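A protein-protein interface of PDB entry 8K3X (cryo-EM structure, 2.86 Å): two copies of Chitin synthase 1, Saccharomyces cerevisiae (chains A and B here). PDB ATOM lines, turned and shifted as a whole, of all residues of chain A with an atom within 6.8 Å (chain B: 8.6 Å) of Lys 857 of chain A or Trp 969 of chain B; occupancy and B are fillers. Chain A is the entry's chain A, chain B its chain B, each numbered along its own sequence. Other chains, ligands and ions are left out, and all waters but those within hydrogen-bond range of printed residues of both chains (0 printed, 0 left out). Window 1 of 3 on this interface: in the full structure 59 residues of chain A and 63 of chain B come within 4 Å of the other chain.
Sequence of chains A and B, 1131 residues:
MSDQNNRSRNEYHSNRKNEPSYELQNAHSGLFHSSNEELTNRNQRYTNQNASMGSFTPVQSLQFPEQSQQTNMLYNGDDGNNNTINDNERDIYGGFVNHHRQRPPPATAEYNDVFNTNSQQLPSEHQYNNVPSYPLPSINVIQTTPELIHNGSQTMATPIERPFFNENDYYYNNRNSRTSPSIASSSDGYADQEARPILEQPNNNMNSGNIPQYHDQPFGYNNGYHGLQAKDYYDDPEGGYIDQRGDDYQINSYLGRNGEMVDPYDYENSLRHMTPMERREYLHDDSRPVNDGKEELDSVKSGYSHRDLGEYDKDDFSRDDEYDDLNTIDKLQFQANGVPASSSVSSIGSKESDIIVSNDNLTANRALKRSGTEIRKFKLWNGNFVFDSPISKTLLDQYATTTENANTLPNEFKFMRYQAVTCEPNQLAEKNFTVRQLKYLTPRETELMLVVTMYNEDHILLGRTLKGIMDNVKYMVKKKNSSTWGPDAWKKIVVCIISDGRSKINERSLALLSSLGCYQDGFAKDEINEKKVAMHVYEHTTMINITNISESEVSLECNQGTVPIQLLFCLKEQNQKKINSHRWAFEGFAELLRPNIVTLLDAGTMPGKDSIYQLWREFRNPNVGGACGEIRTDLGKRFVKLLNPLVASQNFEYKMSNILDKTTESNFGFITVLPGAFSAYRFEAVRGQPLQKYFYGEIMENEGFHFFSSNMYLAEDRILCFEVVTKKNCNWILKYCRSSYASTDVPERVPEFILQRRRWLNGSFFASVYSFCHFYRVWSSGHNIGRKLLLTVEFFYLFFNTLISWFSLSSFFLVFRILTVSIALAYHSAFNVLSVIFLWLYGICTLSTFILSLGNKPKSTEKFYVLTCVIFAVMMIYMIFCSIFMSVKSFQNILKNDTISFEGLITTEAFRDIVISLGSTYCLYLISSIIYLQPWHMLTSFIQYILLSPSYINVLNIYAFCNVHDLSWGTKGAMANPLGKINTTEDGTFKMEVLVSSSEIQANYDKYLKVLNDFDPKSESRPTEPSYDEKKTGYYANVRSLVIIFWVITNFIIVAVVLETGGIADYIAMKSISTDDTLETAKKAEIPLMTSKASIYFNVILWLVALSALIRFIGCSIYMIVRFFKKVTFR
Printed residues of chain A that touch a printed residue of chain B: Leu 852, Asn 856, Lys 857 and Ser 860.
Hydrophobic or aromatic side chains of chain A within 4 Å of the printed part of chain B: Leu 852.
Printed residues of chain B that touch a printed residue of chain A: Trp 969, Gly 1034, Ala 1037, Asn 1038 and Ser 1041.
Among the printed residues, 9 pairs touch across the chains.
Among the printed residues, pairs that only touch across the chains: Ser 860 of chain A with Trp 969 of chain B, Leu 852 of chain A with Ser 1041 of chain B, Asn 856 of chain A with Trp 969 of chain B, Lys 857 of chain A with Trp 969 of chain B, Ser 860 of chain A with Gly 1034 of chain B and Asn 856 of chain A with Ser 1041 of chain B.
The backbone carbonyl oxygen of Gly 1034 of chain B sits close to the side-chain amide oxygen of Asn 1038 of chain B, 3.1 Å away.
The backbone carbonyl oxygen (O) of Ala 1037 of chain B sits at hydrogen-bond distance from the side-chain hydroxyl (OG) of Ser 1041 of chain B (3.0 Å).
1 position is printed for both chains.
Of the 9 pairs that touch across the chains among the printed residues, none has its exchanged pair printed and touching as well.
ND2 of Asn 856 of chain A is in hydrogen-bond range of OD1 of Asn 1038 of chain B (2.7 Å).
The side-chain amide nitrogen (ND2) of Asn 856 of chain A lies within hydrogen-bond range of the backbone carbonyl oxygen (O) of Ala 1037 of chain B, at 3.4 Å.
The backbone carbonyl oxygen of Ser 860 of chain A lies within hydrogen-bond range of the side-chain amide nitrogen of Asn 1038 of chain B (3.3 Å).
Asn 856 of chain A touches just these residues of chain B: Trp 969 (3.5 Å), Ala 1037 (3.4 Å), Asn 1038 (2.7 Å) and Ser 1041 (3.9 Å).
Lys 857 of chain A touches just one residue of chain B: Trp 969.
No residue of chain B comes within 4 Å of Pro 858 of chain A.
Printed residues of chain A within 4 Å of Trp 969 of chain B: Asn 856, Lys 857 and Ser 860.
Printed residues of chain A within 4 Å of Gly 1034 of chain B: Ser 860.
Of the printed residues of chain A, Ala 1037 of chain B touches Asn 856 (3.4 Å).
Printed residues of chain A within 4 Å of Ser 1041 of chain B: Leu 852 and Asn 856.
The nearest residue of chain B that does not touch Lys 857 of chain A is Asn 1038 of chain B (5.8 Å).
The nearest printed residue of chain A that does not touch Trp 969 of chain B is Gly 855 of chain A (4.02 Å).
The nearest printed residue of chain A that does not touch Gly 1034 of chain B is Asn 856 of chain A (5.1 Å).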
ATOM      1  N   LEU A 755     -13.499 -38.067  28.924  1.00  0.00           N
ATOM      2  CA  LEU A 755     -14.695 -38.883  29.059  1.00  0.00           C
ATOM      3  C   LEU A 755     -14.359 -40.306  29.467  1.00  0.00           C
ATOM      4  O   LEU A 755     -15.145 -40.945  30.168  1.00  0.00           O
ATOM      5  CB  LEU A 755     -15.483 -38.877  27.760  1.00  0.00           C
ATOM      6  CG  LEU A 755     -16.205 -37.575  27.469  1.00  0.00           C
ATOM      7  CD1 LEU A 755     -16.561 -37.524  26.020  1.00  0.00           C
ATOM      8  CD2 LEU A 755     -17.433 -37.491  28.311  1.00  0.00           C
ATOM      9  N   LEU A 852     -17.409 -25.306  33.309  1.00  0.00           N
ATOM     10  CA  LEU A 852     -17.568 -26.051  32.071  1.00  0.00           C
ATOM     11  C   LEU A 852     -17.909 -27.508  32.313  1.00  0.00           C
ATOM     12  O   LEU A 852     -18.599 -28.115  31.496  1.00  0.00           O
ATOM     13  CB  LEU A 852     -16.301 -25.962  31.242  1.00  0.00           C
ATOM     14  CG  LEU A 852     -16.027 -24.609  30.629  1.00  0.00           C
ATOM     15  CD1 LEU A 852     -14.820 -24.717  29.786  1.00  0.00           C
ATOM     16  CD2 LEU A 852     -17.188 -24.188  29.801  1.00  0.00           C
ATOM     17  N   SER A 853     -17.421 -28.110  33.392  1.00  0.00           N
ATOM     18  CA  SER A 853     -17.757 -29.503  33.614  1.00  0.00           C
ATOM     19  C   SER A 853     -19.142 -29.660  34.211  1.00  0.00           C
ATOM     20  O   SER A 853     -19.813 -30.655  33.939  1.00  0.00           O
ATOM     21  CB  SER A 853     -16.724 -30.151  34.513  1.00  0.00           C
ATOM     22  OG  SER A 853     -17.034 -29.886  35.855  1.00  0.00           O
ATOM     23  N   GLY A 855     -21.705 -27.547  33.607  1.00  0.00           N
ATOM     24  CA  GLY A 855     -22.731 -27.157  32.662  1.00  0.00           C
ATOM     25  C   GLY A 855     -22.599 -27.693  31.252  1.00  0.00           C
ATOM     26  O   GLY A 855     -23.594 -28.066  30.634  1.00  0.00           O
ATOM     27  N   ASN A 856     -21.388 -27.742  30.735  1.00  0.00           N
ATOM     28  CA  ASN A 856     -21.122 -27.987  29.332  1.00  0.00           C
ATOM     29  C   ASN A 856     -20.656 -29.427  29.116  1.00  0.00           C
ATOM     30  O   ASN A 856     -20.745 -30.271  30.009  1.00  0.00           O
ATOM     31  CB  ASN A 856     -20.103 -26.963  28.855  1.00  0.00           C
ATOM     32  CG  ASN A 856     -20.253 -26.631  27.417  1.00  0.00           C
ATOM     33  OD1 ASN A 856     -20.824 -27.396  26.653  1.00  0.00           O
ATOM     34  ND2 ASN A 856     -19.744 -25.481  27.025  1.00  0.00           N
ATOM     35  N   LYS A 857     -20.176 -29.724  27.911  1.00  0.00           N
ATOM     36  CA  LYS A 857     -19.634 -31.025  27.554  1.00  0.00           C
ATOM     37  C   LYS A 857     -18.247 -30.862  26.955  1.00  0.00           C
ATOM     38  O   LYS A 857     -17.957 -29.841  26.329  1.00  0.00           O
ATOM     39  CB  LYS A 857     -20.535 -31.747  26.547  1.00  0.00           C
ATOM     40  CG  LYS A 857     -21.896 -32.092  27.089  1.00  0.00           C
ATOM     41  CD  LYS A 857     -21.784 -32.898  28.360  1.00  0.00           C
ATOM     42  CE  LYS A 857     -23.095 -33.566  28.701  1.00  0.00           C
ATOM     43  NZ  LYS A 857     -23.424 -34.627  27.729  1.00  0.00           N
ATOM     44  N   PRO A 858     -17.366 -31.848  27.135  1.00  0.00           N
ATOM     45  CA  PRO A 858     -15.989 -31.690  26.657  1.00  0.00           C
ATOM     46  C   PRO A 858     -15.872 -31.552  25.158  1.00  0.00           C
ATOM     47  O   PRO A 858     -14.919 -30.927  24.682  1.00  0.00           O
ATOM     48  CB  PRO A 858     -15.301 -32.965  27.151  1.00  0.00           C
ATOM     49  CG  PRO A 858     -16.163 -33.493  28.182  1.00  0.00           C
ATOM     50  CD  PRO A 858     -17.548 -33.132  27.816  1.00  0.00           C
ATOM     51  N   LYS A 859     -16.790 -32.136  24.393  1.00  0.00           N
ATOM     52  CA  LYS A 859     -16.711 -32.044  22.939  1.00  0.00           C
ATOM     53  C   LYS A 859     -17.004 -30.632  22.454  1.00  0.00           C
ATOM     54  O   LYS A 859     -16.417 -30.174  21.469  1.00  0.00           O
ATOM     55  CB  LYS A 859     -17.681 -33.033  22.312  1.00  0.00           C
ATOM     56  CG  LYS A 859     -17.437 -34.466  22.718  1.00  0.00           C
ATOM     57  CD  LYS A 859     -16.234 -35.041  22.000  1.00  0.00           C
ATOM     58  CE  LYS A 859     -15.996 -36.487  22.401  1.00  0.00           C
ATOM     59  NZ  LYS A 859     -17.092 -37.389  21.960  1.00  0.00           N
ATOM     60  N   SER A 860     -17.921 -29.931  23.124  1.00  0.00           N
ATOM     61  CA  SER A 860     -18.272 -28.576  22.719  1.00  0.00           C
ATOM     62  C   SER A 860     -17.089 -27.635  22.849  1.00  0.00           C
ATOM     63  O   SER A 860     -16.893 -26.752  22.011  1.00  0.00           O
ATOM     64  CB  SER A 860     -19.441 -28.063  23.555  1.00  0.00           C
ATOM     65  OG  SER A 860     -20.644 -28.709  23.200  1.00  0.00           O
ATOM     66  N   THR A 861     -16.295 -27.798  23.901  1.00  0.00           N
ATOM     67  CA  THR A 861     -15.175 -26.911  24.199  1.00  0.00           C
ATOM     68  C   THR A 861     -13.904 -27.736  24.370  1.00  0.00           C
ATOM     69  O   THR A 861     -13.572 -28.188  25.464  1.00  0.00           O
ATOM     70  CB  THR A 861     -15.490 -26.059  25.427  1.00  0.00           C
ATOM     71  OG1 THR A 861     -14.353 -25.260  25.760  1.00  0.00           O
ATOM     72  CG2 THR A 861     -15.932 -26.897  26.619  1.00  0.00           C
ATOM     73  N   GLU A 862     -13.179 -27.935  23.279  1.00  0.00           N
ATOM     74  CA  GLU A 862     -11.922 -28.664  23.318  1.00  0.00           C
ATOM     75  C   GLU A 862     -10.716 -27.742  23.329  1.00  0.00           C
ATOM     76  O   GLU A 862      -9.706 -28.047  23.976  1.00  0.00           O
ATOM     77  CB  GLU A 862     -11.833 -29.604  22.122  1.00  0.00           C
ATOM     78  CG  GLU A 862     -10.477 -30.210  21.916  1.00  0.00           C
ATOM     79  CD  GLU A 862     -10.394 -30.996  20.635  1.00  0.00           C
ATOM     80  OE1 GLU A 862      -9.283 -31.114  20.081  1.00  0.00           O
ATOM     81  OE2 GLU A 862     -11.442 -31.496  20.181  1.00  0.00           O
ATOM     82  N   TYR A 865      -9.899 -26.926  26.916  1.00  0.00           N
ATOM     83  CA  TYR A 865      -9.248 -27.964  27.705  1.00  0.00           C
ATOM     84  C   TYR A 865      -7.793 -28.125  27.304  1.00  0.00           C
ATOM     85  O   TYR A 865      -6.930 -28.338  28.161  1.00  0.00           O
ATOM     86  CB  TYR A 865      -9.999 -29.277  27.568  1.00  0.00           C
ATOM     87  CG  TYR A 865     -11.230 -29.336  28.419  1.00  0.00           C
ATOM     88  CD1 TYR A 865     -11.178 -29.048  29.762  1.00  0.00           C
ATOM     89  CD2 TYR A 865     -12.443 -29.673  27.881  1.00  0.00           C
ATOM     90  CE1 TYR A 865     -12.301 -29.102  30.542  1.00  0.00           C
ATOM     91  CE2 TYR A 865     -13.566 -29.722  28.652  1.00  0.00           C
ATOM     92  CZ  TYR A 865     -13.490 -29.439  29.979  1.00  0.00           C
ATOM     93  OH  TYR A 865     -14.622 -29.500  30.738  1.00  0.00           O
ATOM     94  N   TYR A 959     -13.653 -32.873  36.631  1.00  0.00           N
ATOM     95  CA  TYR A 959     -14.658 -33.385  35.713  1.00  0.00           C
ATOM     96  C   TYR A 959     -15.261 -34.681  36.228  1.00  0.00           C
ATOM     97  O   TYR A 959     -16.448 -34.938  36.028  1.00  0.00           O
ATOM     98  CB  TYR A 959     -14.056 -33.586  34.328  1.00  0.00           C
ATOM     99  CG  TYR A 959     -15.078 -33.958  33.291  1.00  0.00           C
ATOM    100  CD1 TYR A 959     -15.431 -35.268  33.075  1.00  0.00           C
ATOM    101  CD2 TYR A 959     -15.697 -32.993  32.536  1.00  0.00           C
ATOM    102  CE1 TYR A 959     -16.366 -35.601  32.146  1.00  0.00           C
ATOM    103  CE2 TYR A 959     -16.631 -33.320  31.603  1.00  0.00           C
ATOM    104  CZ  TYR A 959     -16.960 -34.625  31.412  1.00  0.00           C
ATOM    105  OH  TYR A 959     -17.899 -34.963  30.477  1.00  0.00           O
ATOM    106  N   ASN A 963     -19.466 -34.907  37.376  1.00  0.00           N
ATOM    107  CA  ASN A 963     -20.304 -35.651  36.443  1.00  0.00           C
ATOM    108  C   ASN A 963     -20.488 -37.084  36.902  1.00  0.00           C
ATOM    109  O   ASN A 963     -20.274 -38.029  36.146  1.00  0.00           O
ATOM    110  CB  ASN A 963     -19.716 -35.631  35.050  1.00  0.00           C
ATOM    111  CG  ASN A 963     -19.922 -34.326  34.374  1.00  0.00           C
ATOM    112  OD1 ASN A 963     -20.814 -33.575  34.729  1.00  0.00           O
ATOM    113  ND2 ASN A 963     -19.118 -34.048  33.376  1.00  0.00           N
ATOM    114  N   ASP A 966     -24.301 -38.934  35.207  1.00  0.00           N
ATOM    115  CA  ASP A 966     -24.775 -38.824  33.824  1.00  0.00           C
ATOM    116  C   ASP A 966     -26.302 -38.693  33.777  1.00  0.00           C
ATOM    117  O   ASP A 966     -27.029 -39.580  33.328  1.00  0.00           O
ATOM    118  CB  ASP A 966     -24.296 -40.018  32.991  1.00  0.00           C
ATOM    119  CG  ASP A 966     -24.676 -39.902  31.534  1.00  0.00           C
ATOM    120  OD1 ASP A 966     -25.046 -38.794  31.098  1.00  0.00           O
ATOM    121  OD2 ASP A 966     -24.603 -40.923  30.819  1.00  0.00           O
ATOM    122  N   ASP B 966     -31.533 -22.781  29.041  1.00  0.00           N
ATOM    123  CA  ASP B 966     -32.404 -23.952  29.186  1.00  0.00           C
ATOM    124  C   ASP B 966     -32.049 -25.030  28.154  1.00  0.00           C
ATOM    125  O   ASP B 966     -32.799 -25.328  27.223  1.00  0.00           O
ATOM    126  CB  ASP B 966     -33.878 -23.547  29.078  1.00  0.00           C
ATOM    127  CG  ASP B 966     -34.820 -24.704  29.319  1.00  0.00           C
ATOM    128  OD1 ASP B 966     -34.371 -25.740  29.847  1.00  0.00           O
ATOM    129  OD2 ASP B 966     -36.014 -24.576  28.979  1.00  0.00           O
ATOM    130  N   LEU B 967     -30.860 -25.594  28.345  1.00  0.00           N
ATOM    131  CA  LEU B 967     -30.280 -26.530  27.396  1.00  0.00           C
ATOM    132  C   LEU B 967     -30.985 -27.880  27.458  1.00  0.00           C
ATOM    133  O   LEU B 967     -31.607 -28.244  28.457  1.00  0.00           O
ATOM    134  CB  LEU B 967     -28.795 -26.735  27.679  1.00  0.00           C
ATOM    135  CG  LEU B 967     -27.815 -25.702  27.128  1.00  0.00           C
ATOM    136  CD1 LEU B 967     -27.852 -25.698  25.645  1.00  0.00           C
ATOM    137  CD2 LEU B 967     -28.081 -24.325  27.652  1.00  0.00           C
ATOM    138  N   SER B 968     -30.871 -28.630  26.364  1.00  0.00           N
ATOM    139  CA  SER B 968     -31.403 -29.990  26.289  1.00  0.00           C
ATOM    140  C   SER B 968     -30.504 -30.761  25.331  1.00  0.00           C
ATOM    141  O   SER B 968     -30.646 -30.639  24.112  1.00  0.00           O
ATOM    142  CB  SER B 968     -32.851 -30.000  25.822  1.00  0.00           C
ATOM    143  OG  SER B 968     -32.965 -29.473  24.513  1.00  0.00           O
ATOM    144  N   TRP B 969     -29.581 -31.544  25.885  1.00  0.00           N
ATOM    145  CA  TRP B 969     -28.553 -32.169  25.066  1.00  0.00           C
ATOM    146  C   TRP B 969     -29.135 -33.287  24.216  1.00  0.00           C
ATOM    147  O   TRP B 969     -29.188 -33.168  22.988  1.00  0.00           O
ATOM    148  CB  TRP B 969     -27.421 -32.690  25.949  1.00  0.00           C
ATOM    149  CG  TRP B 969     -26.586 -31.588  26.504  1.00  0.00           C
ATOM    150  CD1 TRP B 969     -26.692 -31.021  27.735  1.00  0.00           C
ATOM    151  CD2 TRP B 969     -25.528 -30.899  25.834  1.00  0.00           C
ATOM    152  NE1 TRP B 969     -25.759 -30.025  27.878  1.00  0.00           N
ATOM    153  CE2 TRP B 969     -25.033 -29.932  26.722  1.00  0.00           C
ATOM    154  CE3 TRP B 969     -24.949 -31.010  24.571  1.00  0.00           C
ATOM    155  CZ2 TRP B 969     -23.990 -29.085  26.389  1.00  0.00           C
ATOM    156  CZ3 TRP B 969     -23.913 -30.169  24.245  1.00  0.00           C
ATOM    157  CH2 TRP B 969     -23.443 -29.221  25.148  1.00  0.00           C
ATOM    158  N   SER B1027     -26.702 -33.220  13.923  1.00  0.00           N
ATOM    159  CA  SER B1027     -27.917 -32.432  13.757  1.00  0.00           C
ATOM    160  C   SER B1027     -27.710 -30.949  14.020  1.00  0.00           C
ATOM    161  O   SER B1027     -26.939 -30.569  14.906  1.00  0.00           O
ATOM    162  CB  SER B1027     -29.012 -32.957  14.686  1.00  0.00           C
ATOM    163  OG  SER B1027     -29.093 -34.369  14.642  1.00  0.00           O
ATOM    164  N   ASP B1029     -29.767 -29.267  15.482  1.00  0.00           N
ATOM    165  CA  ASP B1029     -30.192 -29.110  16.866  1.00  0.00           C
ATOM    166  C   ASP B1029     -29.029 -29.290  17.827  1.00  0.00           C
ATOM    167  O   ASP B1029     -28.896 -28.536  18.796  1.00  0.00           O
ATOM    168  CB  ASP B1029     -31.313 -30.095  17.188  1.00  0.00           C
ATOM    169  CG  ASP B1029     -32.614 -29.731  16.510  1.00  0.00           C
ATOM    170  OD1 ASP B1029     -32.831 -28.530  16.249  1.00  0.00           O
ATOM    171  OD2 ASP B1029     -33.422 -30.645  16.239  1.00  0.00           O
ATOM    172  N   GLU B1030     -28.171 -30.277  17.582  1.00  0.00           N
ATOM    173  CA  GLU B1030     -27.041 -30.491  18.479  1.00  0.00           C
ATOM    174  C   GLU B1030     -26.012 -29.375  18.359  1.00  0.00           C
ATOM    175  O   GLU B1030     -25.420 -28.962  19.359  1.00  0.00           O
ATOM    176  CB  GLU B1030     -26.403 -31.851  18.214  1.00  0.00           C
ATOM    177  CG  GLU B1030     -27.271 -33.011  18.658  1.00  0.00           C
ATOM    178  CD  GLU B1030     -26.647 -34.355  18.358  1.00  0.00           C
ATOM    179  OE1 GLU B1030     -25.588 -34.383  17.704  1.00  0.00           O
ATOM    180  OE2 GLU B1030     -27.216 -35.383  18.777  1.00  0.00           O
ATOM    181  N   LYS B1031     -25.788 -28.868  17.152  1.00  0.00           N
ATOM    182  CA  LYS B1031     -24.877 -27.740  16.993  1.00  0.00           C
ATOM    183  C   LYS B1031     -25.427 -26.488  17.673  1.00  0.00           C
ATOM    184  O   LYS B1031     -24.678 -25.727  18.303  1.00  0.00           O
ATOM    185  CB  LYS B1031     -24.623 -27.501  15.509  1.00  0.00           C
ATOM    186  CG  LYS B1031     -23.647 -26.403  15.207  1.00  0.00           C
ATOM    187  CD  LYS B1031     -23.059 -26.594  13.827  1.00  0.00           C
ATOM    188  CE  LYS B1031     -24.065 -26.285  12.739  1.00  0.00           C
ATOM    189  NZ  LYS B1031     -24.627 -24.919  12.880  1.00  0.00           N
ATOM    190  N   LYS B1032     -26.734 -26.267  17.570  1.00  0.00           N
ATOM    191  CA  LYS B1032     -27.353 -25.136  18.245  1.00  0.00           C
ATOM    192  C   LYS B1032     -27.263 -25.279  19.757  1.00  0.00           C
ATOM    193  O   LYS B1032     -27.009 -24.300  20.460  1.00  0.00           O
ATOM    194  CB  LYS B1032     -28.801 -25.002  17.795  1.00  0.00           C
ATOM    195  CG  LYS B1032     -29.470 -23.731  18.228  1.00  0.00           C
ATOM    196  CD  LYS B1032     -30.969 -23.823  18.040  1.00  0.00           C
ATOM    197  CE  LYS B1032     -31.560 -24.946  18.867  1.00  0.00           C
ATOM    198  NZ  LYS B1032     -33.042 -24.976  18.792  1.00  0.00           N
ATOM    199  N   THR B1033     -27.472 -26.487  20.277  1.00  0.00           N
ATOM    200  CA  THR B1033     -27.308 -26.713  21.710  1.00  0.00           C
ATOM    201  C   THR B1033     -25.870 -26.491  22.144  1.00  0.00           C
ATOM    202  O   THR B1033     -25.617 -25.957  23.226  1.00  0.00           O
ATOM    203  CB  THR B1033     -27.771 -28.119  22.074  1.00  0.00           C
ATOM    204  OG1 THR B1033     -29.156 -28.266  21.743  1.00  0.00           O
ATOM    205  CG2 THR B1033     -27.570 -28.399  23.531  1.00  0.00           C
ATOM    206  N   GLY B1034     -24.910 -26.884  21.314  1.00  0.00           N
ATOM    207  CA  GLY B1034     -23.523 -26.604  21.635  1.00  0.00           C
ATOM    208  C   GLY B1034     -23.250 -25.121  21.748  1.00  0.00           C
ATOM    209  O   GLY B1034     -22.615 -24.665  22.699  1.00  0.00           O
ATOM    210  N   TYR B1035     -23.742 -24.340  20.787  1.00  0.00           N
ATOM    211  CA  TYR B1035     -23.532 -22.896  20.854  1.00  0.00           C
ATOM    212  C   TYR B1035     -24.213 -22.295  22.072  1.00  0.00           C
ATOM    213  O   TYR B1035     -23.653 -21.423  22.742  1.00  0.00           O
ATOM    214  CB  TYR B1035     -24.045 -22.221  19.591  1.00  0.00           C
ATOM    215  CG  TYR B1035     -24.102 -20.721  19.693  1.00  0.00           C
ATOM    216  CD1 TYR B1035     -22.988 -19.954  19.443  1.00  0.00           C
ATOM    217  CD2 TYR B1035     -25.269 -20.074  20.033  1.00  0.00           C
ATOM    218  CE1 TYR B1035     -23.034 -18.594  19.531  1.00  0.00           C
ATOM    219  CE2 TYR B1035     -25.318 -18.715  20.125  1.00  0.00           C
ATOM    220  CZ  TYR B1035     -24.200 -17.984  19.873  1.00  0.00           C
ATOM    221  OH  TYR B1035     -24.245 -16.625  19.966  1.00  0.00           O
ATOM    222  N   TYR B1036     -25.436 -22.727  22.361  1.00  0.00           N
ATOM    223  CA  TYR B1036     -26.157 -22.171  23.494  1.00  0.00           C
ATOM    224  C   TYR B1036     -25.448 -22.475  24.800  1.00  0.00           C
ATOM    225  O   TYR B1036     -25.354 -21.611  25.674  1.00  0.00           O
ATOM    226  CB  TYR B1036     -27.582 -22.708  23.522  1.00  0.00           C
ATOM    227  CG  TYR B1036     -28.498 -21.987  22.579  1.00  0.00           C
ATOM    228  CD1 TYR B1036     -29.805 -22.386  22.410  1.00  0.00           C
ATOM    229  CD2 TYR B1036     -28.050 -20.904  21.854  1.00  0.00           C
ATOM    230  CE1 TYR B1036     -30.631 -21.725  21.553  1.00  0.00           C
ATOM    231  CE2 TYR B1036     -28.866 -20.242  20.998  1.00  0.00           C
ATOM    232  CZ  TYR B1036     -30.154 -20.653  20.847  1.00  0.00           C
ATOM    233  OH  TYR B1036     -30.975 -19.981  19.981  1.00  0.00           O
ATOM    234  N   ALA B1037     -24.936 -23.689  24.957  1.00  0.00           N
ATOM    235  CA  ALA B1037     -24.233 -24.017  26.184  1.00  0.00           C
ATOM    236  C   ALA B1037     -22.848 -23.406  26.242  1.00  0.00           C
ATOM    237  O   ALA B1037     -22.283 -23.313  27.328  1.00  0.00           O
ATOM    238  CB  ALA B1037     -24.131 -25.526  26.353  1.00  0.00           C
ATOM    239  N   ASN B1038     -22.265 -22.948  25.145  1.00  0.00           N
ATOM    240  CA  ASN B1038     -20.939 -22.284  25.280  1.00  0.00           C
ATOM    241  C   ASN B1038     -21.135 -20.808  25.631  1.00  0.00           C
ATOM    242  O   ASN B1038     -20.189 -20.207  26.131  1.00  0.00           O
ATOM    243  CB  ASN B1038     -20.062 -22.446  24.036  1.00  0.00           C
ATOM    244  CG  ASN B1038     -19.564 -23.858  23.835  1.00  0.00           C
ATOM    245  OD1 ASN B1038     -20.042 -24.785  24.478  1.00  0.00           O
ATOM    246  ND2 ASN B1038     -18.605 -24.028  22.943  1.00  0.00           N
ATOM    247  N   SER B1041     -21.837 -20.525  29.439  1.00  0.00           N
ATOM    248  CA  SER B1041     -20.640 -20.834  30.253  1.00  0.00           C
ATOM    249  C   SER B1041     -19.633 -19.706  30.149  1.00  0.00           C
ATOM    250  O   SER B1041     -18.687 -19.709  30.924  1.00  0.00           O
ATOM    251  CB  SER B1041     -20.021 -22.114  29.814  1.00  0.00           C
ATOM    252  OG  SER B1041     -20.921 -23.195  29.983  1.00  0.00           O
